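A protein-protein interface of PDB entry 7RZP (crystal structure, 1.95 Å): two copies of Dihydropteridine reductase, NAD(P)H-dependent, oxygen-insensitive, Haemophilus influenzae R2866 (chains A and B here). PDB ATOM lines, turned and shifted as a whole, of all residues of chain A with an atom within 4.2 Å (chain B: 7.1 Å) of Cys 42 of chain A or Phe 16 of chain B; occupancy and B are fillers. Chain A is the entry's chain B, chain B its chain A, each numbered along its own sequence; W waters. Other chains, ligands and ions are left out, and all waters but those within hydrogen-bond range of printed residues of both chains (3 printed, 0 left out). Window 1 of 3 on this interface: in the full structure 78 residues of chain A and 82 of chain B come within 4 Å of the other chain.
The side-chain hydroxyl (OG1) of Thr 157 of chain B is in hydrogen-bond range of the side-chain amide oxygen (OD1) of Asn 154 of chain A (3.2 Å).
The side-chain amino group of Lys 210 of chain B lies within hydrogen-bond range of the backbone carbonyl oxygen of Leu 45 of chain A (3.4 Å).
The backbone carbonyl oxygen of Arg 44 of chain A lies close to the guanidinium group of Arg 212 of chain B (3.4 Å).
The guanidinium group (NH2) of Arg 212 of chain B is in hydrogen-bond range of the backbone carbonyl oxygen (O) of Leu 45 of chain A (2.9 Å).
O of Ser 46 of chain A is in hydrogen-bond range of NE of Arg 212 of chain B, 3.1 Å away.
CG1 of Val 12 of chain B touches SG of Cys 38 of chain A, at 3.9 Å.
Glu 41 of chain A touches Leu 13 of chain B (CB to CD2, 3.4 Å).
Glu 41 of chain A touches Leu 215 of chain B (OE2 to CD2, 3.6 Å).
Cys 42 of chain A touches Val 12 of chain B.
Phe 16 of chain B touches Cys 42 of chain A (CD2 to SG, 3.5 Å).
Leu 215 of chain B touches Arg 44 of chain A.
CD2 of Leu 45 of chain A touches ND1 of His 17 of chain B, at 3.9 Å.
Leu 45 of chain A touches Arg 19 of chain B (O to NH2, 3.9 Å).
Asn 154 of chain A touches Phe 16 of chain B.
Gly 158 of chain A touches Phe 16 of chain B (CA to CE2, 3.9 Å).
Of the printed residues of chain B, Glu 41 of chain A touches Leu 13 (3.4 Å) and Leu 215 (3.6 Å).
Cys 42 of chain A touches just these residues of chain B: Val 12 (3.7 Å) and Phe 16 (3.5 Å).
Of the printed residues of chain B, Gly 158 of chain A touches Phe 16.
Of the printed residues of chain A, Arg 19 of chain B touches Leu 45.
Printed residues of chain A within 4 Å of Leu 215 of chain B: Glu 41 and Arg 44.
The nearest residue of chain B that does not touch Cys 42 of chain A is Leu 13 of chain B (5.2 Å).
Water W2 lies within hydrogen-bond range of OD1 of Asn 154 of chain A, OD1 of Asn 154 of chain B and OG1 of Thr 157 of chain B.
Water W3 lies within hydrogen-bond range of the side-chain amide oxygen of Asn 154 of chain A, the backbone carbonyl oxygen of Ala 153 of chain B and the side-chain hydroxyl of Thr 157 of chain B.
Water W1 bridges O of Ser 46 of chain A (3.1 Å) and NE of Arg 212 of chain B (3.4 Å).
1 position is printed for both chains.
Of the 16 pairs that touch across the chains among the printed residues, none has its exchanged pair printed and touching as well.
The backbone carbonyl oxygen (O) of Phe 16 of chain B is in hydrogen-bond range of the side-chain amino group (NZ) of Lys 210 of chain B, 3.2 Å away.
The backbone carbonyl oxygen (O) of Arg 19 of chain B is in hydrogen-bond range of the side-chain amino group (NZ) of Lys 210 of chain B, at 3.0 Å.
The guanidinium group of Arg 44 of chain A is in salt-bridge range of the side-chain carboxylate of Glu 41 of chain A (2.8 Å).
The backbone carbonyl oxygen (O) of Cys 42 of chain A lies within hydrogen-bond range of the side-chain hydroxyl (OG) of Ser 46 of chain A.
The backbone carbonyl oxygen (O) of Gly 43 of chain A lies within hydrogen-bond range of the side-chain hydroxyl (OG) of Ser 46 of chain A.
OG of Ser 46 of chain A sits at hydrogen-bond distance from ND2 of Asn 154 of chain A (2.6 Å).
Of the 11 printed residues of chain A, 8 touch a printed residue of chain B.
Hydrophobic or aromatic side chains of chain A within 4 Å of the printed part of chain B: Leu 45.
Along chain A the printed residues that touch a printed residue of chain B span positions 38 to 158.
Of the 17 printed residues of chain B, 10 touch a printed residue of chain A.
Along chain B the printed residues that touch a printed residue of chain A span positions 12 to 215.
Among the printed residues, no Asp or Glu carboxylate lies within 4 Å of a Lys or Arg side-chain nitrogen of the other chain.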
ATOM      1  N   CYS A  38       1.186 -12.240   2.823  1.00  0.00           N
ATOM      2  CA  CYS A  38       1.513 -12.522   1.426  1.00  0.00           C
ATOM      3  C   CYS A  38       0.507 -13.492   0.819  1.00  0.00           C
ATOM      4  O   CYS A  38       0.004 -13.264  -0.293  1.00  0.00           O
ATOM      5  CB  CYS A  38       2.946 -13.061   1.313  1.00  0.00           C
ATOM      6  SG  CYS A  38       3.553 -13.225  -0.408  1.00  0.00           S
ATOM      7  N   ILE A  39       0.162 -14.555   1.556  1.00  0.00           N
ATOM      8  CA  ILE A  39      -0.804 -15.530   1.061  1.00  0.00           C
ATOM      9  C   ILE A  39      -2.149 -14.861   0.769  1.00  0.00           C
ATOM     10  O   ILE A  39      -2.758 -15.078  -0.288  1.00  0.00           O
ATOM     11  CB  ILE A  39      -0.947 -16.691   2.062  1.00  0.00           C
ATOM     12  CG1 ILE A  39       0.355 -17.504   2.121  1.00  0.00           C
ATOM     13  CG2 ILE A  39      -2.074 -17.588   1.653  1.00  0.00           C
ATOM     14  CD1 ILE A  39       0.321 -18.612   3.161  1.00  0.00           C
ATOM     15  N   LEU A  40      -2.619 -14.023   1.698  1.00  0.00           N
ATOM     16  CA  LEU A  40      -3.853 -13.268   1.481  1.00  0.00           C
ATOM     17  C   LEU A  40      -3.755 -12.378   0.242  1.00  0.00           C
ATOM     18  O   LEU A  40      -4.716 -12.276  -0.537  1.00  0.00           O
ATOM     19  CB  LEU A  40      -4.189 -12.435   2.726  1.00  0.00           C
ATOM     20  CG  LEU A  40      -4.555 -13.255   3.976  1.00  0.00           C
ATOM     21  CD1 LEU A  40      -4.599 -12.380   5.197  1.00  0.00           C
ATOM     22  CD2 LEU A  40      -5.905 -13.966   3.795  1.00  0.00           C
ATOM     23  N   GLU A  41      -2.602 -11.742   0.030  1.00  0.00           N
ATOM     24  CA  GLU A  41      -2.438 -10.916  -1.165  1.00  0.00           C
ATOM     25  C   GLU A  41      -2.592 -11.735  -2.448  1.00  0.00           C
ATOM     26  O   GLU A  41      -3.104 -11.222  -3.460  1.00  0.00           O
ATOM     27  CB  GLU A  41      -1.085 -10.215  -1.132  1.00  0.00           C
ATOM     28  CG  GLU A  41      -0.933  -9.181   0.009  1.00  0.00           C
ATOM     29  CD  GLU A  41      -1.490  -7.814  -0.363  1.00  0.00           C
ATOM     30  OE1 GLU A  41      -2.360  -7.749  -1.256  1.00  0.00           O
ATOM     31  OE2 GLU A  41      -1.048  -6.799   0.217  1.00  0.00           O
ATOM     32  N   CYS A  42      -2.193 -13.018  -2.435  1.00  0.00           N
ATOM     33  CA  CYS A  42      -2.381 -13.821  -3.640  1.00  0.00           C
ATOM     34  C   CYS A  42      -3.851 -13.914  -3.993  1.00  0.00           C
ATOM     35  O   CYS A  42      -4.223 -13.857  -5.177  1.00  0.00           O
ATOM     36  CB  CYS A  42      -1.785 -15.213  -3.458  1.00  0.00           C
ATOM     37  SG  CYS A  42      -0.039 -15.104  -3.162  1.00  0.00           S
ATOM     38  N   GLY A  43      -4.706 -14.033  -2.978  1.00  0.00           N
ATOM     39  CA  GLY A  43      -6.136 -14.073  -3.230  1.00  0.00           C
ATOM     40  C   GLY A  43      -6.713 -12.716  -3.586  1.00  0.00           C
ATOM     41  O   GLY A  43      -7.600 -12.618  -4.429  1.00  0.00           O
ATOM     42  N   ARG A  44      -6.229 -11.649  -2.948  1.00  0.00           N
ATOM     43  CA  ARG A  44      -6.766 -10.326  -3.262  1.00  0.00           C
ATOM     44  C   ARG A  44      -6.450  -9.923  -4.705  1.00  0.00           C
ATOM     45  O   ARG A  44      -7.306  -9.362  -5.407  1.00  0.00           O
ATOM     46  CB  ARG A  44      -6.227  -9.286  -2.274  1.00  0.00           C
ATOM     47  CG  ARG A  44      -6.805  -7.890  -2.515  1.00  0.00           C
ATOM     48  CD  ARG A  44      -6.311  -6.904  -1.479  1.00  0.00           C
ATOM     49  NE  ARG A  44      -4.911  -6.557  -1.675  1.00  0.00           N
ATOM     50  CZ  ARG A  44      -4.456  -5.561  -2.420  1.00  0.00           C
ATOM     51  NH1 ARG A  44      -5.270  -4.762  -3.079  1.00  0.00           N
ATOM     52  NH2 ARG A  44      -3.148  -5.333  -2.468  1.00  0.00           N
ATOM     53  N   LEU A  45      -5.248 -10.256  -5.178  1.00  0.00           N
ATOM     54  CA  LEU A  45      -4.797  -9.921  -6.517  1.00  0.00           C
ATOM     55  C   LEU A  45      -5.342 -10.864  -7.582  1.00  0.00           C
ATOM     56  O   LEU A  45      -5.033 -10.666  -8.765  1.00  0.00           O
ATOM     57  CB  LEU A  45      -3.262  -9.892  -6.555  1.00  0.00           C
ATOM     58  CG  LEU A  45      -2.597  -8.801  -5.710  1.00  0.00           C
ATOM     59  CD1 LEU A  45      -1.111  -9.056  -5.523  1.00  0.00           C
ATOM     60  CD2 LEU A  45      -2.813  -7.444  -6.361  1.00  0.00           C
ATOM     61  N   SER A  46      -6.169 -11.846  -7.211  1.00  0.00           N
ATOM     62  CA  SER A  46      -6.665 -12.789  -8.198  1.00  0.00           C
ATOM     63  C   SER A  46      -7.579 -12.098  -9.203  1.00  0.00           C
ATOM     64  O   SER A  46      -8.281 -11.126  -8.867  1.00  0.00           O
ATOM     65  CB  SER A  46      -7.420 -13.956  -7.541  1.00  0.00           C
ATOM     66  OG  SER A  46      -6.515 -14.754  -6.799  1.00  0.00           O
ATOM     67  N   ASN A 154      -5.012 -19.536  -6.045  1.00  0.00           N
ATOM     68  CA  ASN A 154      -3.842 -18.679  -5.955  1.00  0.00           C
ATOM     69  C   ASN A 154      -3.299 -18.619  -4.536  1.00  0.00           C
ATOM     70  O   ASN A 154      -2.077 -18.550  -4.352  1.00  0.00           O
ATOM     71  CB  ASN A 154      -4.176 -17.287  -6.485  1.00  0.00           C
ATOM     72  CG  ASN A 154      -4.437 -17.301  -7.957  1.00  0.00           C
ATOM     73  OD1 ASN A 154      -3.901 -18.136  -8.684  1.00  0.00           O
ATOM     74  ND2 ASN A 154      -5.266 -16.399  -8.413  1.00  0.00           N
ATOM     75  N   GLY A 158       0.455 -19.693  -3.952  1.00  0.00           N
ATOM     76  CA  GLY A 158       1.370 -18.753  -3.328  1.00  0.00           C
ATOM     77  C   GLY A 158       1.978 -19.297  -2.044  1.00  0.00           C
ATOM     78  O   GLY A 158       3.181 -19.158  -1.811  1.00  0.00           O
ATOM     79  N   GLN B  11       8.928 -11.865  -4.410  1.00  0.00           N
ATOM     80  CA  GLN B  11       8.806 -12.585  -5.683  1.00  0.00           C
ATOM     81  C   GLN B  11       7.393 -13.135  -5.879  1.00  0.00           C
ATOM     82  O   GLN B  11       6.845 -13.077  -6.987  1.00  0.00           O
ATOM     83  CB  GLN B  11       9.842 -13.718  -5.742  1.00  0.00           C
ATOM     84  CG  GLN B  11      11.286 -13.235  -5.976  1.00  0.00           C
ATOM     85  CD  GLN B  11      12.320 -14.348  -5.815  1.00  0.00           C
ATOM     86  OE1 GLN B  11      12.149 -15.244  -4.987  1.00  0.00           O
ATOM     87  NE2 GLN B  11      13.404 -14.283  -6.588  1.00  0.00           N
ATOM     88  N   VAL B  12       6.797 -13.699  -4.819  1.00  0.00           N
ATOM     89  CA  VAL B  12       5.442 -14.239  -4.914  1.00  0.00           C
ATOM     90  C   VAL B  12       4.450 -13.127  -5.222  1.00  0.00           C
ATOM     91  O   VAL B  12       3.562 -13.284  -6.064  1.00  0.00           O
ATOM     92  CB  VAL B  12       5.067 -14.981  -3.617  1.00  0.00           C
ATOM     93  CG1 VAL B  12       3.590 -15.413  -3.636  1.00  0.00           C
ATOM     94  CG2 VAL B  12       5.993 -16.171  -3.379  1.00  0.00           C
ATOM     95  N   LEU B  13       4.579 -11.992  -4.530  1.00  0.00           N
ATOM     96  CA  LEU B  13       3.731 -10.832  -4.804  1.00  0.00           C
ATOM     97  C   LEU B  13       3.868 -10.392  -6.257  1.00  0.00           C
ATOM     98  O   LEU B  13       2.865 -10.165  -6.944  1.00  0.00           O
ATOM     99  CB  LEU B  13       4.101  -9.680  -3.871  1.00  0.00           C
ATOM    100  CG  LEU B  13       3.292  -9.398  -2.597  1.00  0.00           C
ATOM    101  CD1 LEU B  13       3.418  -7.923  -2.228  1.00  0.00           C
ATOM    102  CD2 LEU B  13       1.841  -9.795  -2.743  1.00  0.00           C
ATOM    103  N   GLU B  14       5.101 -10.299  -6.759  1.00  0.00           N
ATOM    104  CA  GLU B  14       5.286  -9.863  -8.141  1.00  0.00           C
ATOM    105  C   GLU B  14       4.643 -10.838  -9.132  1.00  0.00           C
ATOM    106  O   GLU B  14       4.058 -10.419 -10.135  1.00  0.00           O
ATOM    107  CB  GLU B  14       6.768  -9.703  -8.432  1.00  0.00           C
ATOM    108  CG  GLU B  14       7.074  -9.037  -9.732  1.00  0.00           C
ATOM    109  CD  GLU B  14       6.345  -7.713  -9.885  1.00  0.00           C
ATOM    110  OE1 GLU B  14       6.248  -6.953  -8.883  1.00  0.00           O
ATOM    111  OE2 GLU B  14       5.927  -7.404 -11.023  1.00  0.00           O
ATOM    112  N   LEU B  15       4.761 -12.141  -8.869  1.00  0.00           N
ATOM    113  CA  LEU B  15       4.176 -13.170  -9.728  1.00  0.00           C
ATOM    114  C   LEU B  15       2.667 -12.996  -9.880  1.00  0.00           C
ATOM    115  O   LEU B  15       2.126 -13.090 -10.991  1.00  0.00           O
ATOM    116  CB  LEU B  15       4.501 -14.557  -9.155  1.00  0.00           C
ATOM    117  CG  LEU B  15       3.925 -15.782  -9.887  1.00  0.00           C
ATOM    118  CD1 LEU B  15       4.582 -15.984 -11.266  1.00  0.00           C
ATOM    119  CD2 LEU B  15       4.055 -17.016  -9.045  1.00  0.00           C
ATOM    120  N   PHE B  16       1.963 -12.753  -8.774  1.00  0.00           N
ATOM    121  CA  PHE B  16       0.524 -12.582  -8.866  1.00  0.00           C
ATOM    122  C   PHE B  16       0.165 -11.170  -9.263  1.00  0.00           C
ATOM    123  O   PHE B  16      -0.908 -10.957  -9.821  1.00  0.00           O
ATOM    124  CB  PHE B  16      -0.157 -12.971  -7.551  1.00  0.00           C
ATOM    125  CG  PHE B  16      -0.214 -14.438  -7.350  1.00  0.00           C
ATOM    126  CD1 PHE B  16      -1.181 -15.196  -7.993  1.00  0.00           C
ATOM    127  CD2 PHE B  16       0.755 -15.079  -6.609  1.00  0.00           C
ATOM    128  CE1 PHE B  16      -1.199 -16.567  -7.880  1.00  0.00           C
ATOM    129  CE2 PHE B  16       0.741 -16.468  -6.475  1.00  0.00           C
ATOM    130  CZ  PHE B  16      -0.248 -17.215  -7.108  1.00  0.00           C
ATOM    131  N   HIS B  17       1.070 -10.220  -9.042  1.00  0.00           N
ATOM    132  CA  HIS B  17       0.875  -8.853  -9.517  1.00  0.00           C
ATOM    133  C   HIS B  17       1.152  -8.701 -11.009  1.00  0.00           C
ATOM    134  O   HIS B  17       0.514  -7.867 -11.675  1.00  0.00           O
ATOM    135  CB  HIS B  17       1.775  -7.887  -8.744  1.00  0.00           C
ATOM    136  CG  HIS B  17       1.258  -6.490  -8.727  1.00  0.00           C
ATOM    137  ND1 HIS B  17       0.521  -5.985  -7.676  1.00  0.00           N
ATOM    138  CD2 HIS B  17       1.327  -5.506  -9.653  1.00  0.00           C
ATOM    139  CE1 HIS B  17       0.175  -4.739  -7.949  1.00  0.00           C
ATOM    140  NE2 HIS B  17       0.654  -4.421  -9.140  1.00  0.00           N
ATOM    141  N   GLN B  18       2.121  -9.453 -11.544  1.00  0.00           N
ATOM    142  CA  GLN B  18       2.479  -9.312 -12.952  1.00  0.00           C
ATOM    143  C   GLN B  18       1.450  -9.948 -13.886  1.00  0.00           C
ATOM    144  O   GLN B  18       1.364  -9.533 -15.043  1.00  0.00           O
ATOM    145  CB  GLN B  18       3.890  -9.877 -13.222  1.00  0.00           C
ATOM    146  CG  GLN B  18       4.008 -11.409 -13.324  1.00  0.00           C
ATOM    147  CD  GLN B  18       5.449 -11.925 -13.162  1.00  0.00           C
ATOM    148  OE1 GLN B  18       6.301 -11.264 -12.570  1.00  0.00           O
ATOM    149  NE2 GLN B  18       5.701 -13.132 -13.654  1.00  0.00           N
ATOM    150  N   ARG B  19       0.669 -10.940 -13.426  1.00  0.00           N
ATOM    151  CA  ARG B  19      -0.382 -11.539 -14.263  1.00  0.00           C
ATOM    152  C   ARG B  19      -1.575 -10.606 -14.426  1.00  0.00           C
ATOM    153  O   ARG B  19      -2.238 -10.254 -13.449  1.00  0.00           O
ATOM    154  CB  ARG B  19      -0.813 -12.897 -13.719  1.00  0.00           C
ATOM    155  CG  ARG B  19      -1.787 -13.617 -14.687  1.00  0.00           C
ATOM    156  CD  ARG B  19      -3.066 -13.970 -13.942  1.00  0.00           C
ATOM    157  NE  ARG B  19      -3.593 -12.839 -13.174  1.00  0.00           N
ATOM    158  CZ  ARG B  19      -4.577 -12.027 -13.531  1.00  0.00           C
ATOM    159  NH1 ARG B  19      -5.134 -12.096 -14.743  1.00  0.00           N
ATOM    160  NH2 ARG B  19      -5.008 -11.116 -12.647  1.00  0.00           N
ATOM    161  N   SER B  20      -1.822 -10.172 -15.663  1.00  0.00           N
ATOM    162  CA  SER B  20      -2.906  -9.254 -15.980  1.00  0.00           C
ATOM    163  C   SER B  20      -3.713  -9.858 -17.120  1.00  0.00           C
ATOM    164  O   SER B  20      -3.297 -10.837 -17.756  1.00  0.00           O
ATOM    165  CB  SER B  20      -2.369  -7.873 -16.353  1.00  0.00           C
ATOM    166  OG  SER B  20      -2.341  -7.025 -15.217  1.00  0.00           O
ATOM    167  N   ALA B 153      -7.093 -21.151 -12.826  1.00  0.00           N
ATOM    168  CA  ALA B 153      -6.223 -20.189 -12.147  1.00  0.00           C
ATOM    169  C   ALA B 153      -4.770 -20.635 -12.196  1.00  0.00           C
ATOM    170  O   ALA B 153      -3.869 -19.818 -12.415  1.00  0.00           O
ATOM    171  CB  ALA B 153      -6.654 -19.969 -10.694  1.00  0.00           C
ATOM    172  N   ASN B 154      -4.522 -21.934 -12.038  1.00  0.00           N
ATOM    173  CA  ASN B 154      -3.133 -22.379 -12.022  1.00  0.00           C
ATOM    174  C   ASN B 154      -2.516 -22.296 -13.407  1.00  0.00           C
ATOM    175  O   ASN B 154      -1.304 -22.097 -13.534  1.00  0.00           O
ATOM    176  CB  ASN B 154      -3.060 -23.792 -11.448  1.00  0.00           C
ATOM    177  CG  ASN B 154      -3.375 -23.805  -9.940  1.00  0.00           C
ATOM    178  OD1 ASN B 154      -3.028 -22.870  -9.221  1.00  0.00           O
ATOM    179  ND2 ASN B 154      -4.031 -24.849  -9.470  1.00  0.00           N
ATOM    180  N   THR B 157      -1.462 -18.561 -13.711  1.00  0.00           N
ATOM    181  CA  THR B 157      -0.262 -18.314 -12.922  1.00  0.00           C
ATOM    182  C   THR B 157       0.944 -19.004 -13.539  1.00  0.00           C
ATOM    183  O   THR B 157       2.029 -18.415 -13.622  1.00  0.00           O
ATOM    184  CB  THR B 157      -0.504 -18.787 -11.493  1.00  0.00           C
ATOM    185  OG1 THR B 157      -1.751 -18.241 -11.041  1.00  0.00           O
ATOM    186  CG2 THR B 157       0.607 -18.353 -10.573  1.00  0.00           C
ATOM    187  N   SER B 160       2.103 -17.116 -16.517  1.00  0.00           N
ATOM    188  CA  SER B 160       2.801 -15.928 -16.043  1.00  0.00           C
ATOM    189  C   SER B 160       4.233 -16.238 -15.636  1.00  0.00           C
ATOM    190  O   SER B 160       5.166 -15.512 -16.004  1.00  0.00           O
ATOM    191  CB  SER B 160       2.040 -15.330 -14.870  1.00  0.00           C
ATOM    192  OG  SER B 160       2.728 -14.205 -14.364  1.00  0.00           O
ATOM    193  N   LYS B 210      -3.107  -2.832 -12.002  1.00  0.00           N
ATOM    194  CA  LYS B 210      -4.012  -3.635 -11.202  1.00  0.00           C
ATOM    195  C   LYS B 210      -4.956  -2.674 -10.485  1.00  0.00           C
ATOM    196  O   LYS B 210      -4.561  -1.566 -10.110  1.00  0.00           O
ATOM    197  CB  LYS B 210      -3.260  -4.508 -10.178  1.00  0.00           C
ATOM    198  CG  LYS B 210      -3.477  -6.010 -10.346  1.00  0.00           C
ATOM    199  CD  LYS B 210      -2.914  -6.459 -11.683  1.00  0.00           C
ATOM    200  CE  LYS B 210      -3.313  -7.864 -12.048  1.00  0.00           C
ATOM    201  NZ  LYS B 210      -3.185  -8.939 -10.963  1.00  0.00           N
ATOM    202  N   ARG B 212      -7.774  -3.262  -7.375  1.00  0.00           N
ATOM    203  CA  ARG B 212      -8.418  -4.234  -6.496  1.00  0.00           C
ATOM    204  C   ARG B 212      -8.967  -3.526  -5.270  1.00  0.00           C
ATOM    205  O   ARG B 212      -8.556  -2.412  -4.936  1.00  0.00           O
ATOM    206  CB  ARG B 212      -7.454  -5.335  -6.028  1.00  0.00           C
ATOM    207  CG  ARG B 212      -6.997  -6.303  -7.091  1.00  0.00           C
ATOM    208  CD  ARG B 212      -8.132  -7.157  -7.668  1.00  0.00           C
ATOM    209  NE  ARG B 212      -7.587  -8.169  -8.565  1.00  0.00           N
ATOM    210  CZ  ARG B 212      -7.231  -7.960  -9.831  1.00  0.00           C
ATOM    211  NH1 ARG B 212      -7.394  -6.778 -10.421  1.00  0.00           N
ATOM    212  NH2 ARG B 212      -6.656  -8.946 -10.511  1.00  0.00           N
ATOM    213  N   LEU B 215      -6.741  -4.630   1.029  1.00  0.00           N
ATOM    214  CA  LEU B 215      -6.648  -5.808   1.886  1.00  0.00           C
ATOM    215  C   LEU B 215      -7.576  -5.688   3.099  1.00  0.00           C
ATOM    216  O   LEU B 215      -8.180  -6.679   3.531  1.00  0.00           O
ATOM    217  CB  LEU B 215      -5.189  -6.014   2.297  1.00  0.00           C
ATOM    218  CG  LEU B 215      -4.813  -7.402   2.807  1.00  0.00           C
ATOM    219  CD1 LEU B 215      -5.276  -8.474   1.853  1.00  0.00           C
ATOM    220  CD2 LEU B 215      -3.299  -7.471   3.006  1.00  0.00           C
HETATM  221  O   HOH W   1     -10.293  -9.292 -10.307  1.00  0.00           O
HETATM  222  O   HOH W   2      -2.324 -20.208  -9.101  1.00  0.00           O
HETATM  223  O   HOH W   3      -4.570 -17.082 -11.406  1.00  0.00           O
